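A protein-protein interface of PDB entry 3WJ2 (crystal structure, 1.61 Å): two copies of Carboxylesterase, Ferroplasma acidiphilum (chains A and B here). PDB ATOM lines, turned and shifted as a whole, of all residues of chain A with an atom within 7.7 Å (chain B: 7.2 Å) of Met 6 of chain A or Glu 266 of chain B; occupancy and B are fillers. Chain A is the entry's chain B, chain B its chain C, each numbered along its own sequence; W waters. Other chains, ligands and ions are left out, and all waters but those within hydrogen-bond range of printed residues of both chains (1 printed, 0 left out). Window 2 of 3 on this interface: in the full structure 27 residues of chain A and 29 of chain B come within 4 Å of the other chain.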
ATOM      1  N   ASN A   5      18.337  11.671   8.233  1.00  0.00           N
ATOM      2  CA  ASN A   5      19.095  12.237   9.409  1.00  0.00           C
ATOM      3  C   ASN A   5      18.394  13.524   9.843  1.00  0.00           C
ATOM      4  O   ASN A   5      17.196  13.482  10.119  1.00  0.00           O
ATOM      5  CB  ASN A   5      20.567  12.472   9.112  1.00  0.00           C
ATOM      6  CG  ASN A   5      21.288  11.230   8.603  1.00  0.00           C
ATOM      7  OD1 ASN A   5      21.860  11.241   7.491  1.00  0.00           O
ATOM      8  ND2 ASN A   5      21.212  10.118   9.382  1.00  0.00           N
ATOM      9  N   MET A   6      19.082  14.668   9.997  1.00  0.00           N
ATOM     10  CA  MET A   6      18.361  15.856  10.364  1.00  0.00           C
ATOM     11  C   MET A   6      18.422  16.947   9.238  1.00  0.00           C
ATOM     12  O   MET A   6      18.693  18.117   9.508  1.00  0.00           O
ATOM     13  CB  MET A   6      18.923  16.432  11.634  1.00  0.00           C
ATOM     14  CG  MET A   6      18.666  15.527  12.831  1.00  0.00           C
ATOM     15  SD  MET A   6      16.909  15.331  13.288  1.00  0.00           S
ATOM     16  CE  MET A   6      16.385  16.748  14.221  1.00  0.00           C
ATOM     17  N   VAL A   7      18.227  16.481   8.006  1.00  0.00           N
ATOM     18  CA  VAL A   7      18.139  17.438   6.821  1.00  0.00           C
ATOM     19  C   VAL A   7      17.090  18.506   7.146  1.00  0.00           C
ATOM     20  O   VAL A   7      15.963  18.214   7.670  1.00  0.00           O
ATOM     21  CB  VAL A   7      17.828  16.622   5.551  1.00  0.00           C
ATOM     22  CG1 VAL A   7      17.533  17.613   4.370  1.00  0.00           C
ATOM     23  CG2 VAL A   7      19.012  15.746   5.090  1.00  0.00           C
ATOM     24  N   ASP A   8      17.338  19.785   6.855  1.00  0.00           N
ATOM     25  CA  ASP A   8      16.408  20.888   7.177  1.00  0.00           C
ATOM     26  C   ASP A   8      15.051  20.562   6.422  1.00  0.00           C
ATOM     27  O   ASP A   8      15.078  20.168   5.248  1.00  0.00           O
ATOM     28  CB  ASP A   8      16.991  22.218   6.591  1.00  0.00           C
ATOM     29  CG  ASP A   8      16.192  23.396   6.970  1.00  0.00           C
ATOM     30  OD1 ASP A   8      14.923  23.417   6.672  1.00  0.00           O
ATOM     31  OD2 ASP A   8      16.661  24.338   7.612  1.00  0.00           O
ATOM     32  N   PRO A   9      13.936  20.626   7.169  1.00  0.00           N
ATOM     33  CA  PRO A   9      12.682  20.134   6.530  1.00  0.00           C
ATOM     34  C   PRO A   9      12.251  20.955   5.356  1.00  0.00           C
ATOM     35  O   PRO A   9      11.423  20.409   4.522  1.00  0.00           O
ATOM     36  CB  PRO A   9      11.671  20.192   7.652  1.00  0.00           C
ATOM     37  CG  PRO A   9      12.600  19.979   8.978  1.00  0.00           C
ATOM     38  CD  PRO A   9      13.859  20.752   8.617  1.00  0.00           C
ATOM     39  N   PHE A  11      13.841  21.205   2.767  1.00  0.00           N
ATOM     40  CA  PHE A  11      14.209  20.442   1.550  1.00  0.00           C
ATOM     41  C   PHE A  11      13.341  19.191   1.298  1.00  0.00           C
ATOM     42  O   PHE A  11      13.626  18.462   0.373  1.00  0.00           O
ATOM     43  CB  PHE A  11      15.689  19.987   1.632  1.00  0.00           C
ATOM     44  CG  PHE A  11      16.620  21.168   1.710  1.00  0.00           C
ATOM     45  CD1 PHE A  11      16.744  22.020   0.614  1.00  0.00           C
ATOM     46  CD2 PHE A  11      17.398  21.384   2.862  1.00  0.00           C
ATOM     47  CE1 PHE A  11      17.613  23.164   0.632  1.00  0.00           C
ATOM     48  CE2 PHE A  11      18.264  22.548   2.932  1.00  0.00           C
ATOM     49  CZ  PHE A  11      18.376  23.400   1.798  1.00  0.00           C
ATOM     50  N   ASN A  12      12.338  18.930   2.158  1.00  0.00           N
ATOM     51  CA  ASN A  12      11.620  17.653   2.005  1.00  0.00           C
ATOM     52  C   ASN A  12      10.957  17.590   0.607  1.00  0.00           C
ATOM     53  O   ASN A  12      11.074  16.501  -0.038  1.00  0.00           O
ATOM     54  CB  ASN A  12      10.605  17.465   3.141  1.00  0.00           C
ATOM     55  CG  ASN A  12      11.309  17.144   4.493  1.00  0.00           C
ATOM     56  OD1 ASN A  12      12.512  16.835   4.525  1.00  0.00           O
ATOM     57  ND2 ASN A  12      10.549  17.215   5.593  1.00  0.00           N
ATOM     58  N   TYR A 199      25.894   9.875   2.081  1.00  0.00           N
ATOM     59  CA  TYR A 199      24.864  10.796   1.519  1.00  0.00           C
ATOM     60  C   TYR A 199      24.639  10.600   0.021  1.00  0.00           C
ATOM     61  O   TYR A 199      24.060  11.479  -0.606  1.00  0.00           O
ATOM     62  CB  TYR A 199      25.194  12.246   1.862  1.00  0.00           C
ATOM     63  CG  TYR A 199      25.429  12.454   3.292  1.00  0.00           C
ATOM     64  CD1 TYR A 199      24.487  12.006   4.262  1.00  0.00           C
ATOM     65  CD2 TYR A 199      26.615  13.037   3.754  1.00  0.00           C
ATOM     66  CE1 TYR A 199      24.774  12.136   5.583  1.00  0.00           C
ATOM     67  CE2 TYR A 199      26.849  13.210   5.039  1.00  0.00           C
ATOM     68  CZ  TYR A 199      25.920  12.767   5.986  1.00  0.00           C
ATOM     69  OH  TYR A 199      26.213  12.888   7.298  1.00  0.00           O
ATOM     70  N   GLU A 249      26.188  20.196   5.103  1.00  0.00           N
ATOM     71  CA  GLU A 249      26.261  18.957   5.963  1.00  0.00           C
ATOM     72  C   GLU A 249      25.906  17.652   5.287  1.00  0.00           C
ATOM     73  O   GLU A 249      26.660  16.675   5.393  1.00  0.00           O
ATOM     74  CB  GLU A 249      25.357  19.201   7.182  1.00  0.00           C
ATOM     75  CG  GLU A 249      25.535  18.053   8.171  1.00  0.00           C
ATOM     76  CD  GLU A 249      24.790  18.287   9.453  1.00  0.00           C
ATOM     77  OE1 GLU A 249      23.996  19.211   9.607  1.00  0.00           O
ATOM     78  OE2 GLU A 249      25.079  17.496  10.412  1.00  0.00           O
ATOM     79  N   TYR A 250      24.807  17.652   4.524  1.00  0.00           N
ATOM     80  CA  TYR A 250      24.324  16.351   4.008  1.00  0.00           C
ATOM     81  C   TYR A 250      24.507  16.258   2.515  1.00  0.00           C
ATOM     82  O   TYR A 250      23.579  16.419   1.749  1.00  0.00           O
ATOM     83  CB  TYR A 250      22.824  16.318   4.377  1.00  0.00           C
ATOM     84  CG  TYR A 250      22.585  16.164   5.895  1.00  0.00           C
ATOM     85  CD1 TYR A 250      23.024  15.034   6.551  1.00  0.00           C
ATOM     86  CD2 TYR A 250      21.936  17.135   6.590  1.00  0.00           C
ATOM     87  CE1 TYR A 250      22.806  14.928   7.972  1.00  0.00           C
ATOM     88  CE2 TYR A 250      21.629  17.023   7.936  1.00  0.00           C
ATOM     89  CZ  TYR A 250      22.096  15.901   8.604  1.00  0.00           C
ATOM     90  OH  TYR A 250      21.792  15.745   9.944  1.00  0.00           O
ATOM     91  N   ILE A 277      24.634  23.765   8.424  1.00  0.00           N
ATOM     92  CA  ILE A 277      24.031  22.659   9.221  1.00  0.00           C
ATOM     93  C   ILE A 277      22.645  22.359   8.624  1.00  0.00           C
ATOM     94  O   ILE A 277      21.850  23.271   8.368  1.00  0.00           O
ATOM     95  CB  ILE A 277      24.013  23.072  10.661  1.00  0.00           C
ATOM     96  CG1 ILE A 277      25.479  23.070  11.173  1.00  0.00           C
ATOM     97  CG2 ILE A 277      23.231  21.980  11.511  1.00  0.00           C
ATOM     98  CD1 ILE A 277      25.609  23.945  12.445  1.00  0.00           C
ATOM     99  N   GLY A 278      22.416  21.093   8.360  1.00  0.00           N
ATOM    100  CA  GLY A 278      21.130  20.680   7.747  1.00  0.00           C
ATOM    101  C   GLY A 278      21.015  20.927   6.279  1.00  0.00           C
ATOM    102  O   GLY A 278      19.935  20.663   5.696  1.00  0.00           O
ATOM    103  N   MET A 279      22.022  21.482   5.605  1.00  0.00           N
ATOM    104  CA  MET A 279      21.870  21.770   4.184  1.00  0.00           C
ATOM    105  C   MET A 279      22.259  20.587   3.266  1.00  0.00           C
ATOM    106  O   MET A 279      22.958  19.642   3.701  1.00  0.00           O
ATOM    107  CB  MET A 279      22.825  22.931   3.804  1.00  0.00           C
ATOM    108  CG  MET A 279      22.558  24.193   4.610  1.00  0.00           C
ATOM    109  SD  MET A 279      20.970  24.935   3.943  1.00  0.00           S
ATOM    110  CE  MET A 279      19.911  24.803   5.387  1.00  0.00           C
ATOM    111  N   PHE B 237      10.555  23.149  21.687  1.00  0.00           N
ATOM    112  CA  PHE B 237      11.223  24.299  21.022  1.00  0.00           C
ATOM    113  C   PHE B 237      10.358  25.200  20.147  1.00  0.00           C
ATOM    114  O   PHE B 237      10.847  26.115  19.490  1.00  0.00           O
ATOM    115  CB  PHE B 237      12.453  23.780  20.297  1.00  0.00           C
ATOM    116  CG  PHE B 237      13.402  23.170  21.230  1.00  0.00           C
ATOM    117  CD1 PHE B 237      14.097  23.977  22.134  1.00  0.00           C
ATOM    118  CD2 PHE B 237      13.471  21.770  21.365  1.00  0.00           C
ATOM    119  CE1 PHE B 237      14.971  23.405  23.058  1.00  0.00           C
ATOM    120  CE2 PHE B 237      14.315  21.182  22.267  1.00  0.00           C
ATOM    121  CZ  PHE B 237      15.086  22.013  23.161  1.00  0.00           C
ATOM    122  N   GLU B 258      25.005  21.776  17.432  1.00  0.00           N
ATOM    123  CA  GLU B 258      24.407  21.365  16.136  1.00  0.00           C
ATOM    124  C   GLU B 258      23.052  20.678  16.337  1.00  0.00           C
ATOM    125  O   GLU B 258      22.137  20.885  15.587  1.00  0.00           O
ATOM    126  CB  GLU B 258      25.466  20.533  15.312  1.00  0.00           C
ATOM    127  CG  GLU B 258      26.725  21.438  15.086  1.00  0.00           C
ATOM    128  CD  GLU B 258      27.803  20.884  14.151  1.00  0.00           C
ATOM    129  OE1 GLU B 258      27.739  19.677  13.739  1.00  0.00           O
ATOM    130  OE2 GLU B 258      28.684  21.682  13.791  1.00  0.00           O
ATOM    131  N   THR B 259      22.945  19.894  17.412  1.00  0.00           N
ATOM    132  CA  THR B 259      21.671  19.279  17.752  1.00  0.00           C
ATOM    133  C   THR B 259      20.611  20.359  18.000  1.00  0.00           C
ATOM    134  O   THR B 259      19.502  20.236  17.525  1.00  0.00           O
ATOM    135  CB  THR B 259      21.845  18.413  19.008  1.00  0.00           C
ATOM    136  OG1 THR B 259      22.663  17.242  18.625  1.00  0.00           O
ATOM    137  CG2 THR B 259      20.358  17.937  19.466  1.00  0.00           C
ATOM    138  N   TYR B 260      21.007  21.398  18.729  1.00  0.00           N
ATOM    139  CA  TYR B 260      20.101  22.462  19.118  1.00  0.00           C
ATOM    140  C   TYR B 260      19.507  23.116  17.868  1.00  0.00           C
ATOM    141  O   TYR B 260      18.290  23.350  17.776  1.00  0.00           O
ATOM    142  CB  TYR B 260      20.738  23.512  19.980  1.00  0.00           C
ATOM    143  CG  TYR B 260      19.741  24.382  20.730  1.00  0.00           C
ATOM    144  CD1 TYR B 260      19.064  23.845  21.809  1.00  0.00           C
ATOM    145  CD2 TYR B 260      19.636  25.727  20.453  1.00  0.00           C
ATOM    146  CE1 TYR B 260      18.144  24.632  22.585  1.00  0.00           C
ATOM    147  CE2 TYR B 260      18.677  26.568  21.174  1.00  0.00           C
ATOM    148  CZ  TYR B 260      17.942  25.962  22.221  1.00  0.00           C
ATOM    149  OH  TYR B 260      17.135  26.737  22.992  1.00  0.00           O
ATOM    150  N   VAL B 261      20.348  23.448  16.889  1.00  0.00           N
ATOM    151  CA  VAL B 261      19.798  24.087  15.744  1.00  0.00           C
ATOM    152  C   VAL B 261      18.872  23.111  14.947  1.00  0.00           C
ATOM    153  O   VAL B 261      17.844  23.569  14.463  1.00  0.00           O
ATOM    154  CB  VAL B 261      20.993  24.844  15.032  1.00  0.00           C
ATOM    155  CG1 VAL B 261      21.555  23.935  14.210  1.00  0.00           C
ATOM    156  CG2 VAL B 261      20.360  26.117  14.286  1.00  0.00           C
ATOM    157  N   LYS B 262      19.108  21.791  14.956  1.00  0.00           N
ATOM    158  CA  LYS B 262      18.226  20.820  14.306  1.00  0.00           C
ATOM    159  C   LYS B 262      16.902  20.698  15.085  1.00  0.00           C
ATOM    160  O   LYS B 262      15.867  20.568  14.478  1.00  0.00           O
ATOM    161  CB  LYS B 262      18.857  19.450  14.223  1.00  0.00           C
ATOM    162  CG  LYS B 262      20.099  19.410  13.182  1.00  0.00           C
ATOM    163  CD  LYS B 262      21.100  18.286  13.450  1.00  0.00           C
ATOM    164  CE  LYS B 262      22.123  18.362  12.252  1.00  0.00           C
ATOM    165  NZ  LYS B 262      23.164  17.349  12.373  1.00  0.00           N
ATOM    166  N   LYS B 263      16.999  20.744  16.400  1.00  0.00           N
ATOM    167  CA  LYS B 263      15.723  20.750  17.219  1.00  0.00           C
ATOM    168  C   LYS B 263      14.896  22.028  17.001  1.00  0.00           C
ATOM    169  O   LYS B 263      13.667  21.935  16.893  1.00  0.00           O
ATOM    170  CB  LYS B 263      16.044  20.589  18.700  1.00  0.00           C
ATOM    171  CG  LYS B 263      16.697  19.233  19.090  1.00  0.00           C
ATOM    172  CD  LYS B 263      15.756  18.149  18.832  1.00  0.00           C
ATOM    173  CE  LYS B 263      14.496  18.395  19.706  1.00  0.00           C
ATOM    174  NZ  LYS B 263      13.658  17.174  19.790  1.00  0.00           N
ATOM    175  N   LEU B 264      15.521  23.205  16.854  1.00  0.00           N
ATOM    176  CA  LEU B 264      14.761  24.412  16.438  1.00  0.00           C
ATOM    177  C   LEU B 264      14.067  24.264  15.152  1.00  0.00           C
ATOM    178  O   LEU B 264      12.868  24.565  15.028  1.00  0.00           O
ATOM    179  CB  LEU B 264      15.684  25.621  16.425  1.00  0.00           C
ATOM    180  CG  LEU B 264      16.344  26.035  17.704  1.00  0.00           C
ATOM    181  CD1 LEU B 264      17.304  27.283  17.467  1.00  0.00           C
ATOM    182  CD2 LEU B 264      15.258  26.349  18.709  1.00  0.00           C
ATOM    183  N   ARG B 265      14.764  23.738  14.123  1.00  0.00           N
ATOM    184  CA  ARG B 265      14.134  23.574  12.801  1.00  0.00           C
ATOM    185  C   ARG B 265      12.996  22.524  12.883  1.00  0.00           C
ATOM    186  O   ARG B 265      11.978  22.716  12.240  1.00  0.00           O
ATOM    187  CB  ARG B 265      15.181  23.114  11.730  1.00  0.00           C
ATOM    188  CG  ARG B 265      16.134  24.274  11.440  1.00  0.00           C
ATOM    189  CD  ARG B 265      15.431  25.562  10.818  1.00  0.00           C
ATOM    190  NE  ARG B 265      14.784  25.148   9.582  1.00  0.00           N
ATOM    191  CZ  ARG B 265      13.479  25.376   9.359  1.00  0.00           C
ATOM    192  NH1 ARG B 265      12.692  25.968  10.296  1.00  0.00           N
ATOM    193  NH2 ARG B 265      12.961  24.954   8.200  1.00  0.00           N
ATOM    194  N   GLU B 266      13.217  21.480  13.669  1.00  0.00           N
ATOM    195  CA  GLU B 266      12.231  20.366  13.828  1.00  0.00           C
ATOM    196  C   GLU B 266      10.923  20.936  14.408  1.00  0.00           C
ATOM    197  O   GLU B 266       9.769  20.552  13.975  1.00  0.00           O
ATOM    198  CB  GLU B 266      12.806  19.335  14.762  1.00  0.00           C
ATOM    199  CG  GLU B 266      11.844  18.102  14.925  1.00  0.00           C
ATOM    200  CD  GLU B 266      12.435  17.182  15.950  1.00  0.00           C
ATOM    201  OE1 GLU B 266      12.511  17.533  17.198  1.00  0.00           O
ATOM    202  OE2 GLU B 266      12.917  16.120  15.491  1.00  0.00           O
ATOM    203  N   ALA B 267      11.073  21.944  15.244  1.00  0.00           N
ATOM    204  CA  ALA B 267       9.913  22.666  15.834  1.00  0.00           C
ATOM    205  C   ALA B 267       9.309  23.813  14.981  1.00  0.00           C
ATOM    206  O   ALA B 267       8.410  24.544  15.428  1.00  0.00           O
ATOM    207  CB  ALA B 267      10.295  23.168  17.230  1.00  0.00           C
ATOM    208  N   GLY B 268       9.907  24.089  13.818  1.00  0.00           N
ATOM    209  CA  GLY B 268       9.446  25.123  12.886  1.00  0.00           C
ATOM    210  C   GLY B 268       9.911  26.520  13.209  1.00  0.00           C
ATOM    211  O   GLY B 268       9.346  27.505  12.730  1.00  0.00           O
ATOM    212  N   VAL B 269      10.990  26.621  13.993  1.00  0.00           N
ATOM    213  CA  VAL B 269      11.565  27.896  14.280  1.00  0.00           C
ATOM    214  C   VAL B 269      12.605  28.212  13.151  1.00  0.00           C
ATOM    215  O   VAL B 269      13.340  27.263  12.793  1.00  0.00           O
ATOM    216  CB  VAL B 269      12.282  27.791  15.588  1.00  0.00           C
ATOM    217  CG1 VAL B 269      13.108  29.112  15.901  1.00  0.00           C
ATOM    218  CG2 VAL B 269      11.200  27.517  16.766  1.00  0.00           C
HETATM  219  O   HOH W   1      27.341  19.351  10.962  1.00  0.00           O
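OH of Tyr 250 of chain A is in hydrogen-bond range of N of Met 6 of chain A (2.9 Å).
The backbone carbonyl oxygen (O) of Gly 278 of chain A is in hydrogen-bond range of the backbone NH (N) of Asp 8 of chain A, 3.0 Å away.
OE1 of Glu 249 of chain A sits at hydrogen-bond distance from N of Gly 278 of chain A (2.8 Å).
The backbone NH (N) of Tyr 250 of chain A sits at hydrogen-bond distance from the backbone carbonyl oxygen (O) of Met 279 of chain A (2.8 Å).
The side-chain carboxylate (OE1) of Glu 266 of chain B lies within salt-bridge range of the side-chain amino group (NZ) of Lys 263 of chain B, at 2.9 Å.
NH1 of Arg 265 of chain B lies within hydrogen-bond range of O of Val 269 of chain B, 2.9 Å away.
No position is printed for both chains.
Of the 8 pairs that touch across the chains among the printed residues, none has its exchanged pair printed and touching as well.
CD of Lys 262 of chain B touches CB of Met 6 of chain A (3.4 Å).
Glu 266 of chain B touches Met 6 of chain A.
Ile 277 of chain A touches Glu 258 of chain B.
CG2 of Ile 277 of chain A touches CG1 of Val 261 of chain B (3.7 Å).
Ile 277 of chain A touches Lys 262 of chain B.
Of the 13 printed residues of chain B, 5 touch a printed residue of chain A.
Hydrophobic or aromatic side chains of chain B that line the printed part of chain A: Val 261.
Hydrophobic or aromatic side chains of chain A that line the printed part of chain B: Met 6, Tyr 250 and Ile 277.
Among the printed residues, Asp or Glu carboxylates within 4 Å of a Lys or Arg side-chain nitrogen of the other chain: Asp 8 of chain A with Arg 265 of chain B (2.8 Å) and Glu 249 of chain A with Lys 262 of chain B (2.7 Å).
Water W1 bridges OE1 of Glu 258 of chain B (2.8 Å) and OE2 of Glu 249 of chain A (3.0 Å).
Of chain A, only Met 6 comes within 4 Å of Glu 266 of chain B.
Of the printed residues of chain B, Glu 249 of chain A touches Lys 262 (2.7 Å).
Of the printed residues of chain B, Tyr 250 of chain A touches Lys 262.
Of the printed residues of chain B, Asp 8 of chain A touches Arg 265.
Tyr 199 of chain A touches none of the printed residues of chain B.
The nearest residue of chain B that does not touch Met 6 of chain A is Lys 263 of chain B (4.6 Å).
The nearest residue of chain A that does not touch Glu 266 of chain B is Pro 9 of chain A (4.9 Å).
The nearest printed residue of chain B that does not touch Glu 249 of chain A is Glu 258 of chain B (4.8 Å).
The side-chain carboxylate (OD2) of Asp 8 of chain A is in salt-bridge range of the guanidinium group (NE) of Arg 265 of chain B, 2.8 Å away.
The side-chain amino group of Lys 262 of chain B lies within salt-bridge range of the side-chain carboxylate of Glu 249 of chain A.
OH of Tyr 250 of chain A is in hydrogen-bond range of NZ of Lys 262 of chain B (3.2 Å).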
